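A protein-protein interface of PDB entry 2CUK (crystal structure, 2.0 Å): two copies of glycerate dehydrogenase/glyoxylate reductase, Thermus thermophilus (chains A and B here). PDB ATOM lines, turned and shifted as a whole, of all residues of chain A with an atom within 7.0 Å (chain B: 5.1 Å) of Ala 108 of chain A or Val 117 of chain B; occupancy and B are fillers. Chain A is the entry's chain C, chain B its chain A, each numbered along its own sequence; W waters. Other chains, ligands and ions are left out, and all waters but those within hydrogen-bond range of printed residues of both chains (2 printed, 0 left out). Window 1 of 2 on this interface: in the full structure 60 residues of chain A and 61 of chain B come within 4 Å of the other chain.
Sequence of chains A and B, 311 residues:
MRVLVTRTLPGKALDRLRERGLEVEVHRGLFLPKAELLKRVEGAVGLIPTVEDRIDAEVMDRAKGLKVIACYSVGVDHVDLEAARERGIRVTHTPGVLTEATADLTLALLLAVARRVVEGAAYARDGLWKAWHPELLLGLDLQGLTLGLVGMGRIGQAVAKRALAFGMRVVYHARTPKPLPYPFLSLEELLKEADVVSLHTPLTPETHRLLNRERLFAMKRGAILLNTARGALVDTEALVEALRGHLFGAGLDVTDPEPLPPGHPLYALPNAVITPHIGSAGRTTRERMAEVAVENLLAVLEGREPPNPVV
The backbone carbonyl oxygen (O) of Ile 278 of chain A lies within hydrogen-bond range of the guanidinium group (NH2) of Arg 115 of chain B (2.7 Å).
O of Ala 112 of chain B lies within hydrogen-bond range of N of Val 117 of chain B (3.0 Å).
Asp 104 of chain A touches Leu 111 of chain B.
CB of Asp 104 of chain A touches NH1 of Arg 115 of chain B, 3.97 Å away.
Leu 111 of chain B touches Ala 108 of chain A (CB to CB, 3.7 Å).
Ala 108 of chain A touches Val 117 of chain B (CB to CG2, 3.8 Å).
Leu 111 of chain B touches Leu 111 of chain A.
CA of Ala 121 of chain B touches O of Ile 274 of chain A, 3.4 Å away.
O of Gly 120 of chain B touches CD of Pro 276 of chain A, at 3.2 Å.
Of the printed residues of chain B, Ala 108 of chain A touches Leu 111 (3.7 Å) and Val 117 (3.8 Å).
Of chain A, only Ala 108 (3.8 Å) comes within 4 Å of Val 117 of chain B.
Printed residues of chain A within 4 Å of Arg 115 of chain B: Asp 104 and Ile 278.
Of the printed residues of chain B, Leu 111 of chain A touches Leu 111.
The nearest residue of chain A that does not touch Val 117 of chain B is Thr 275 of chain A (4.04 Å).
The nearest printed residue of chain A that does not touch Arg 115 of chain B is Leu 105 of chain A (4.1 Å).
Of the 10 printed residues of chain B, 5 touch a printed residue of chain A.
Printed residues of chain A that touch a printed residue of chain B: Asp 104, Ala 108, Leu 111, Ile 274, Pro 276 and Ile 278.
Among the printed residues, no Asp or Glu carboxylate lies within 4 Å of a Lys or Arg side-chain nitrogen of the other chain.
Leu 111 of chain B touches its own counterpart, Leu 111 of chain A.
Of the 8 pairs that touch across the chains among the printed residues, 1 has its exchanged pair printed and touching as well.
Water W1 bridges OD2 of Asp 104 of chain A and NH1 of Arg 115 of chain B.
Water W2 lies within hydrogen-bond range of O of Ala 121 of chain B and O of Ile 274 of chain A.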
ATOM      1  N   THR A 102      12.586 -12.772   4.168  1.00  0.00           N
ATOM      2  CA  THR A 102      12.580 -14.026   4.905  1.00  0.00           C
ATOM      3  C   THR A 102      13.066 -13.811   6.334  1.00  0.00           C
ATOM      4  O   THR A 102      12.536 -14.401   7.277  1.00  0.00           O
ATOM      5  CB  THR A 102      13.445 -15.071   4.189  1.00  0.00           C
ATOM      6  OG1 THR A 102      13.007 -15.179   2.831  1.00  0.00           O
ATOM      7  CG2 THR A 102      13.317 -16.440   4.865  1.00  0.00           C
ATOM      8  N   ALA A 103      14.060 -12.945   6.496  1.00  0.00           N
ATOM      9  CA  ALA A 103      14.585 -12.653   7.823  1.00  0.00           C
ATOM     10  C   ALA A 103      13.491 -11.979   8.647  1.00  0.00           C
ATOM     11  O   ALA A 103      13.326 -12.279   9.822  1.00  0.00           O
ATOM     12  CB  ALA A 103      15.817 -11.746   7.723  1.00  0.00           C
ATOM     13  N   ASP A 104      12.736 -11.077   8.020  1.00  0.00           N
ATOM     14  CA  ASP A 104      11.651 -10.376   8.704  1.00  0.00           C
ATOM     15  C   ASP A 104      10.588 -11.343   9.228  1.00  0.00           C
ATOM     16  O   ASP A 104      10.139 -11.230  10.367  1.00  0.00           O
ATOM     17  CB  ASP A 104      10.963  -9.377   7.765  1.00  0.00           C
ATOM     18  CG  ASP A 104      11.835  -8.180   7.426  1.00  0.00           C
ATOM     19  OD1 ASP A 104      12.870  -7.974   8.092  1.00  0.00           O
ATOM     20  OD2 ASP A 104      11.469  -7.433   6.496  1.00  0.00           O
ATOM     21  N   LEU A 105      10.181 -12.283   8.381  1.00  0.00           N
ATOM     22  CA  LEU A 105       9.164 -13.261   8.744  1.00  0.00           C
ATOM     23  C   LEU A 105       9.670 -14.172   9.862  1.00  0.00           C
ATOM     24  O   LEU A 105       8.912 -14.553  10.759  1.00  0.00           O
ATOM     25  CB  LEU A 105       8.766 -14.075   7.505  1.00  0.00           C
ATOM     26  CG  LEU A 105       7.574 -15.040   7.561  1.00  0.00           C
ATOM     27  CD1 LEU A 105       7.984 -16.340   8.221  1.00  0.00           C
ATOM     28  CD2 LEU A 105       6.412 -14.390   8.307  1.00  0.00           C
ATOM     29  N   THR A 106      10.954 -14.510   9.815  1.00  0.00           N
ATOM     30  CA  THR A 106      11.546 -15.352  10.846  1.00  0.00           C
ATOM     31  C   THR A 106      11.419 -14.650  12.200  1.00  0.00           C
ATOM     32  O   THR A 106      11.026 -15.262  13.195  1.00  0.00           O
ATOM     33  CB  THR A 106      13.035 -15.633  10.553  1.00  0.00           C
ATOM     34  OG1 THR A 106      13.156 -16.279   9.279  1.00  0.00           O
ATOM     35  CG2 THR A 106      13.633 -16.535  11.633  1.00  0.00           C
ATOM     36  N   LEU A 107      11.748 -13.360  12.237  1.00  0.00           N
ATOM     37  CA  LEU A 107      11.637 -12.596  13.481  1.00  0.00           C
ATOM     38  C   LEU A 107      10.169 -12.450  13.880  1.00  0.00           C
ATOM     39  O   LEU A 107       9.834 -12.460  15.065  1.00  0.00           O
ATOM     40  CB  LEU A 107      12.272 -11.207  13.329  1.00  0.00           C
ATOM     41  CG  LEU A 107      13.745 -11.055  13.737  1.00  0.00           C
ATOM     42  CD1 LEU A 107      13.875 -11.214  15.247  1.00  0.00           C
ATOM     43  CD2 LEU A 107      14.601 -12.087  13.012  1.00  0.00           C
ATOM     44  N   ALA A 108       9.293 -12.313  12.888  1.00  0.00           N
ATOM     45  CA  ALA A 108       7.866 -12.181  13.170  1.00  0.00           C
ATOM     46  C   ALA A 108       7.371 -13.429  13.912  1.00  0.00           C
ATOM     47  O   ALA A 108       6.629 -13.336  14.891  1.00  0.00           O
ATOM     48  CB  ALA A 108       7.087 -11.995  11.864  1.00  0.00           C
ATOM     49  N   LEU A 109       7.796 -14.595  13.439  1.00  0.00           N
ATOM     50  CA  LEU A 109       7.404 -15.858  14.055  1.00  0.00           C
ATOM     51  C   LEU A 109       7.974 -15.995  15.462  1.00  0.00           C
ATOM     52  O   LEU A 109       7.285 -16.467  16.374  1.00  0.00           O
ATOM     53  CB  LEU A 109       7.850 -17.035  13.182  1.00  0.00           C
ATOM     54  CG  LEU A 109       6.976 -17.243  11.941  1.00  0.00           C
ATOM     55  CD1 LEU A 109       7.524 -18.385  11.098  1.00  0.00           C
ATOM     56  CD2 LEU A 109       5.542 -17.544  12.382  1.00  0.00           C
ATOM     57  N   LEU A 110       9.227 -15.580  15.644  1.00  0.00           N
ATOM     58  CA  LEU A 110       9.842 -15.649  16.965  1.00  0.00           C
ATOM     59  C   LEU A 110       9.031 -14.823  17.963  1.00  0.00           C
ATOM     60  O   LEU A 110       8.691 -15.300  19.050  1.00  0.00           O
ATOM     61  CB  LEU A 110      11.284 -15.136  16.916  1.00  0.00           C
ATOM     62  CG  LEU A 110      12.013 -15.026  18.261  1.00  0.00           C
ATOM     63  CD1 LEU A 110      11.929 -16.351  19.013  1.00  0.00           C
ATOM     64  CD2 LEU A 110      13.470 -14.635  18.011  1.00  0.00           C
ATOM     65  N   LEU A 111       8.721 -13.586  17.588  1.00  0.00           N
ATOM     66  CA  LEU A 111       7.948 -12.702  18.452  1.00  0.00           C
ATOM     67  C   LEU A 111       6.527 -13.234  18.654  1.00  0.00           C
ATOM     68  O   LEU A 111       5.978 -13.153  19.750  1.00  0.00           O
ATOM     69  CB  LEU A 111       7.921 -11.281  17.860  1.00  0.00           C
ATOM     70  CG  LEU A 111       9.265 -10.535  17.929  1.00  0.00           C
ATOM     71  CD1 LEU A 111       9.227  -9.273  17.078  1.00  0.00           C
ATOM     72  CD2 LEU A 111       9.584 -10.187  19.370  1.00  0.00           C
ATOM     73  N   ALA A 112       5.938 -13.784  17.597  1.00  0.00           N
ATOM     74  CA  ALA A 112       4.591 -14.336  17.675  1.00  0.00           C
ATOM     75  C   ALA A 112       4.551 -15.480  18.695  1.00  0.00           C
ATOM     76  O   ALA A 112       3.621 -15.578  19.493  1.00  0.00           O
ATOM     77  CB  ALA A 112       4.150 -14.840  16.303  1.00  0.00           C
ATOM     78  N   VAL A 113       5.557 -16.346  18.668  1.00  0.00           N
ATOM     79  CA  VAL A 113       5.597 -17.456  19.619  1.00  0.00           C
ATOM     80  C   VAL A 113       5.992 -16.975  21.014  1.00  0.00           C
ATOM     81  O   VAL A 113       5.247 -17.162  21.982  1.00  0.00           O
ATOM     82  CB  VAL A 113       6.590 -18.554  19.162  1.00  0.00           C
ATOM     83  CG1 VAL A 113       6.684 -19.659  20.215  1.00  0.00           C
ATOM     84  CG2 VAL A 113       6.128 -19.146  17.823  1.00  0.00           C
ATOM     85  N   ALA A 114       7.150 -16.327  21.107  1.00  0.00           N
ATOM     86  CA  ALA A 114       7.664 -15.845  22.384  1.00  0.00           C
ATOM     87  C   ALA A 114       6.672 -14.992  23.159  1.00  0.00           C
ATOM     88  O   ALA A 114       6.543 -15.148  24.371  1.00  0.00           O
ATOM     89  CB  ALA A 114       8.966 -15.071  22.172  1.00  0.00           C
ATOM     90  N   VAL A 117       1.373 -13.813  20.585  1.00  0.00           N
ATOM     91  CA  VAL A 117       0.558 -12.821  19.892  1.00  0.00           C
ATOM     92  C   VAL A 117      -0.668 -13.394  19.181  1.00  0.00           C
ATOM     93  O   VAL A 117      -1.760 -12.832  19.277  1.00  0.00           O
ATOM     94  CB  VAL A 117       1.414 -12.041  18.872  1.00  0.00           C
ATOM     95  CG1 VAL A 117       0.546 -11.060  18.088  1.00  0.00           C
ATOM     96  CG2 VAL A 117       2.529 -11.304  19.602  1.00  0.00           C
ATOM     97  N   VAL A 118      -0.491 -14.503  18.470  1.00  0.00           N
ATOM     98  CA  VAL A 118      -1.603 -15.118  17.749  1.00  0.00           C
ATOM     99  C   VAL A 118      -2.616 -15.622  18.771  1.00  0.00           C
ATOM    100  O   VAL A 118      -3.828 -15.467  18.602  1.00  0.00           O
ATOM    101  CB  VAL A 118      -1.116 -16.290  16.864  1.00  0.00           C
ATOM    102  CG1 VAL A 118      -2.294 -16.918  16.117  1.00  0.00           C
ATOM    103  CG2 VAL A 118      -0.069 -15.782  15.873  1.00  0.00           C
ATOM    104  N   VAL A 273       2.953 -21.765  16.172  1.00  0.00           N
ATOM    105  CA  VAL A 273       2.387 -20.790  15.247  1.00  0.00           C
ATOM    106  C   VAL A 273       2.845 -21.222  13.864  1.00  0.00           C
ATOM    107  O   VAL A 273       4.037 -21.217  13.563  1.00  0.00           O
ATOM    108  CB  VAL A 273       2.891 -19.348  15.526  1.00  0.00           C
ATOM    109  CG1 VAL A 273       2.345 -18.383  14.459  1.00  0.00           C
ATOM    110  CG2 VAL A 273       2.437 -18.896  16.910  1.00  0.00           C
ATOM    111  N   ILE A 274       1.890 -21.625  13.034  1.00  0.00           N
ATOM    112  CA  ILE A 274       2.196 -22.078  11.686  1.00  0.00           C
ATOM    113  C   ILE A 274       1.666 -21.104  10.643  1.00  0.00           C
ATOM    114  O   ILE A 274       0.487 -20.746  10.652  1.00  0.00           O
ATOM    115  CB  ILE A 274       1.575 -23.477  11.404  1.00  0.00           C
ATOM    116  CG1 ILE A 274       2.346 -24.570  12.153  1.00  0.00           C
ATOM    117  CG2 ILE A 274       1.621 -23.783   9.912  1.00  0.00           C
ATOM    118  CD1 ILE A 274       2.239 -24.510  13.648  1.00  0.00           C
ATOM    119  N   THR A 275       2.550 -20.656   9.761  1.00  0.00           N
ATOM    120  CA  THR A 275       2.156 -19.755   8.684  1.00  0.00           C
ATOM    121  C   THR A 275       2.345 -20.551   7.401  1.00  0.00           C
ATOM    122  O   THR A 275       3.233 -21.398   7.312  1.00  0.00           O
ATOM    123  CB  THR A 275       3.002 -18.464   8.666  1.00  0.00           C
ATOM    124  OG1 THR A 275       4.391 -18.786   8.792  1.00  0.00           O
ATOM    125  CG2 THR A 275       2.585 -17.554   9.815  1.00  0.00           C
ATOM    126  N   PRO A 276       1.510 -20.288   6.388  1.00  0.00           N
ATOM    127  CA  PRO A 276       1.557 -20.984   5.102  1.00  0.00           C
ATOM    128  C   PRO A 276       2.703 -20.685   4.134  1.00  0.00           C
ATOM    129  O   PRO A 276       2.466 -20.283   2.998  1.00  0.00           O
ATOM    130  CB  PRO A 276       0.187 -20.670   4.509  1.00  0.00           C
ATOM    131  CG  PRO A 276      -0.039 -19.260   4.969  1.00  0.00           C
ATOM    132  CD  PRO A 276       0.414 -19.298   6.416  1.00  0.00           C
ATOM    133  N   ILE A 278       5.027 -18.272   3.855  1.00  0.00           N
ATOM    134  CA  ILE A 278       5.006 -16.907   3.331  1.00  0.00           C
ATOM    135  C   ILE A 278       6.297 -16.138   3.633  1.00  0.00           C
ATOM    136  O   ILE A 278       6.325 -14.908   3.575  1.00  0.00           O
ATOM    137  CB  ILE A 278       3.817 -16.112   3.918  1.00  0.00           C
ATOM    138  CG1 ILE A 278       3.964 -16.003   5.438  1.00  0.00           C
ATOM    139  CG2 ILE A 278       2.507 -16.793   3.552  1.00  0.00           C
ATOM    140  CD1 ILE A 278       2.812 -15.286   6.131  1.00  0.00           C
ATOM    141  N   LEU B 111       5.191  -6.360  12.626  1.00  0.00           N
ATOM    142  CA  LEU B 111       5.426  -7.506  11.755  1.00  0.00           C
ATOM    143  C   LEU B 111       4.154  -8.315  11.553  1.00  0.00           C
ATOM    144  O   LEU B 111       3.910  -8.830  10.461  1.00  0.00           O
ATOM    145  CB  LEU B 111       6.525  -8.396  12.340  1.00  0.00           C
ATOM    146  CG  LEU B 111       7.938  -7.807  12.311  1.00  0.00           C
ATOM    147  CD1 LEU B 111       8.873  -8.627  13.195  1.00  0.00           C
ATOM    148  CD2 LEU B 111       8.434  -7.786  10.870  1.00  0.00           C
ATOM    149  N   ALA B 112       3.339  -8.420  12.599  1.00  0.00           N
ATOM    150  CA  ALA B 112       2.092  -9.167  12.506  1.00  0.00           C
ATOM    151  C   ALA B 112       1.187  -8.565  11.432  1.00  0.00           C
ATOM    152  O   ALA B 112       0.578  -9.287  10.652  1.00  0.00           O
ATOM    153  CB  ALA B 112       1.378  -9.160  13.845  1.00  0.00           C
ATOM    154  N   ARG B 115       3.214  -8.204   7.661  1.00  0.00           N
ATOM    155  CA  ARG B 115       3.387  -9.459   6.927  1.00  0.00           C
ATOM    156  C   ARG B 115       2.223 -10.436   7.147  1.00  0.00           C
ATOM    157  O   ARG B 115       2.310 -11.624   6.860  1.00  0.00           O
ATOM    158  CB  ARG B 115       4.698 -10.101   7.384  1.00  0.00           C
ATOM    159  CG  ARG B 115       5.910  -9.216   7.095  1.00  0.00           C
ATOM    160  CD  ARG B 115       6.182  -9.085   5.592  1.00  0.00           C
ATOM    161  NE  ARG B 115       6.013 -10.379   4.924  1.00  0.00           N
ATOM    162  CZ  ARG B 115       7.121 -11.116   4.719  1.00  0.00           C
ATOM    163  NH1 ARG B 115       8.299 -10.670   5.118  1.00  0.00           N
ATOM    164  NH2 ARG B 115       7.021 -12.304   4.113  1.00  0.00           N
ATOM    165  N   ARG B 116       1.113  -9.897   7.688  1.00  0.00           N
ATOM    166  CA  ARG B 116      -0.117 -10.684   7.792  1.00  0.00           C
ATOM    167  C   ARG B 116       0.113 -12.043   8.451  1.00  0.00           C
ATOM    168  O   ARG B 116      -0.370 -13.073   8.000  1.00  0.00           O
ATOM    169  CB  ARG B 116      -0.669 -10.880   6.382  1.00  0.00           C
ATOM    170  CG  ARG B 116      -0.810  -9.559   5.627  1.00  0.00           C
ATOM    171  CD  ARG B 116      -1.136  -9.776   4.146  1.00  0.00           C
ATOM    172  NE  ARG B 116      -2.522 -10.223   3.995  1.00  0.00           N
ATOM    173  CZ  ARG B 116      -2.996 -10.344   2.744  1.00  0.00           C
ATOM    174  NH1 ARG B 116      -2.222 -10.066   1.710  1.00  0.00           N
ATOM    175  NH2 ARG B 116      -4.244 -10.780   2.553  1.00  0.00           N
ATOM    176  N   VAL B 117       0.825 -12.042   9.573  1.00  0.00           N
ATOM    177  CA  VAL B 117       1.095 -13.265  10.311  1.00  0.00           C
ATOM    178  C   VAL B 117      -0.152 -13.854  10.985  1.00  0.00           C
ATOM    179  O   VAL B 117      -0.420 -15.048  10.864  1.00  0.00           O
ATOM    180  CB  VAL B 117       2.196 -13.021  11.363  1.00  0.00           C
ATOM    181  CG1 VAL B 117       2.432 -14.281  12.184  1.00  0.00           C
ATOM    182  CG2 VAL B 117       3.484 -12.599  10.661  1.00  0.00           C
ATOM    183  N   VAL B 118      -0.913 -13.031  11.696  1.00  0.00           N
ATOM    184  CA  VAL B 118      -2.113 -13.533  12.357  1.00  0.00           C
ATOM    185  C   VAL B 118      -3.078 -14.051  11.298  1.00  0.00           C
ATOM    186  O   VAL B 118      -3.642 -15.140  11.428  1.00  0.00           O
ATOM    187  CB  VAL B 118      -2.796 -12.437  13.190  1.00  0.00           C
ATOM    188  CG1 VAL B 118      -4.119 -12.951  13.750  1.00  0.00           C
ATOM    189  CG2 VAL B 118      -1.877 -12.010  14.319  1.00  0.00           C
ATOM    190  N   GLU B 119      -3.247 -13.268  10.237  1.00  0.00           N
ATOM    191  CA  GLU B 119      -4.121 -13.639   9.131  1.00  0.00           C
ATOM    192  C   GLU B 119      -3.649 -14.957   8.511  1.00  0.00           C
ATOM    193  O   GLU B 119      -4.449 -15.852   8.245  1.00  0.00           O
ATOM    194  CB  GLU B 119      -4.103 -12.540   8.064  1.00  0.00           C
ATOM    195  CG  GLU B 119      -5.157 -12.699   6.988  1.00  0.00           C
ATOM    196  CD  GLU B 119      -5.012 -11.678   5.864  1.00  0.00           C
ATOM    197  OE1 GLU B 119      -4.437 -10.593   6.104  1.00  0.00           O
ATOM    198  OE2 GLU B 119      -5.486 -11.962   4.745  1.00  0.00           O
ATOM    199  N   GLY B 120      -2.345 -15.061   8.279  1.00  0.00           N
ATOM    200  CA  GLY B 120      -1.783 -16.270   7.696  1.00  0.00           C
ATOM    201  C   GLY B 120      -1.984 -17.502   8.563  1.00  0.00           C
ATOM    202  O   GLY B 120      -2.250 -18.596   8.051  1.00  0.00           O
ATOM    203  N   ALA B 121      -1.852 -17.328   9.879  1.00  0.00           N
ATOM    204  CA  ALA B 121      -2.031 -18.433  10.815  1.00  0.00           C
ATOM    205  C   ALA B 121      -3.467 -18.945  10.746  1.00  0.00           C
ATOM    206  O   ALA B 121      -3.707 -20.149  10.818  1.00  0.00           O
ATOM    207  CB  ALA B 121      -1.702 -17.986  12.234  1.00  0.00           C
ATOM    208  N   ALA B 122      -4.418 -18.029  10.597  1.00  0.00           N
ATOM    209  CA  ALA B 122      -5.824 -18.410  10.508  1.00  0.00           C
ATOM    210  C   ALA B 122      -6.070 -19.152   9.197  1.00  0.00           C
ATOM    211  O   ALA B 122      -6.801 -20.144   9.155  1.00  0.00           O
ATOM    212  CB  ALA B 122      -6.708 -17.172  10.579  1.00  0.00           C
HETATM  213  O   HOH W   1       9.274  -7.651   4.991  1.00  0.00           O
HETATM  214  O   HOH W   2      -1.805 -21.794  11.720  1.00  0.00           O
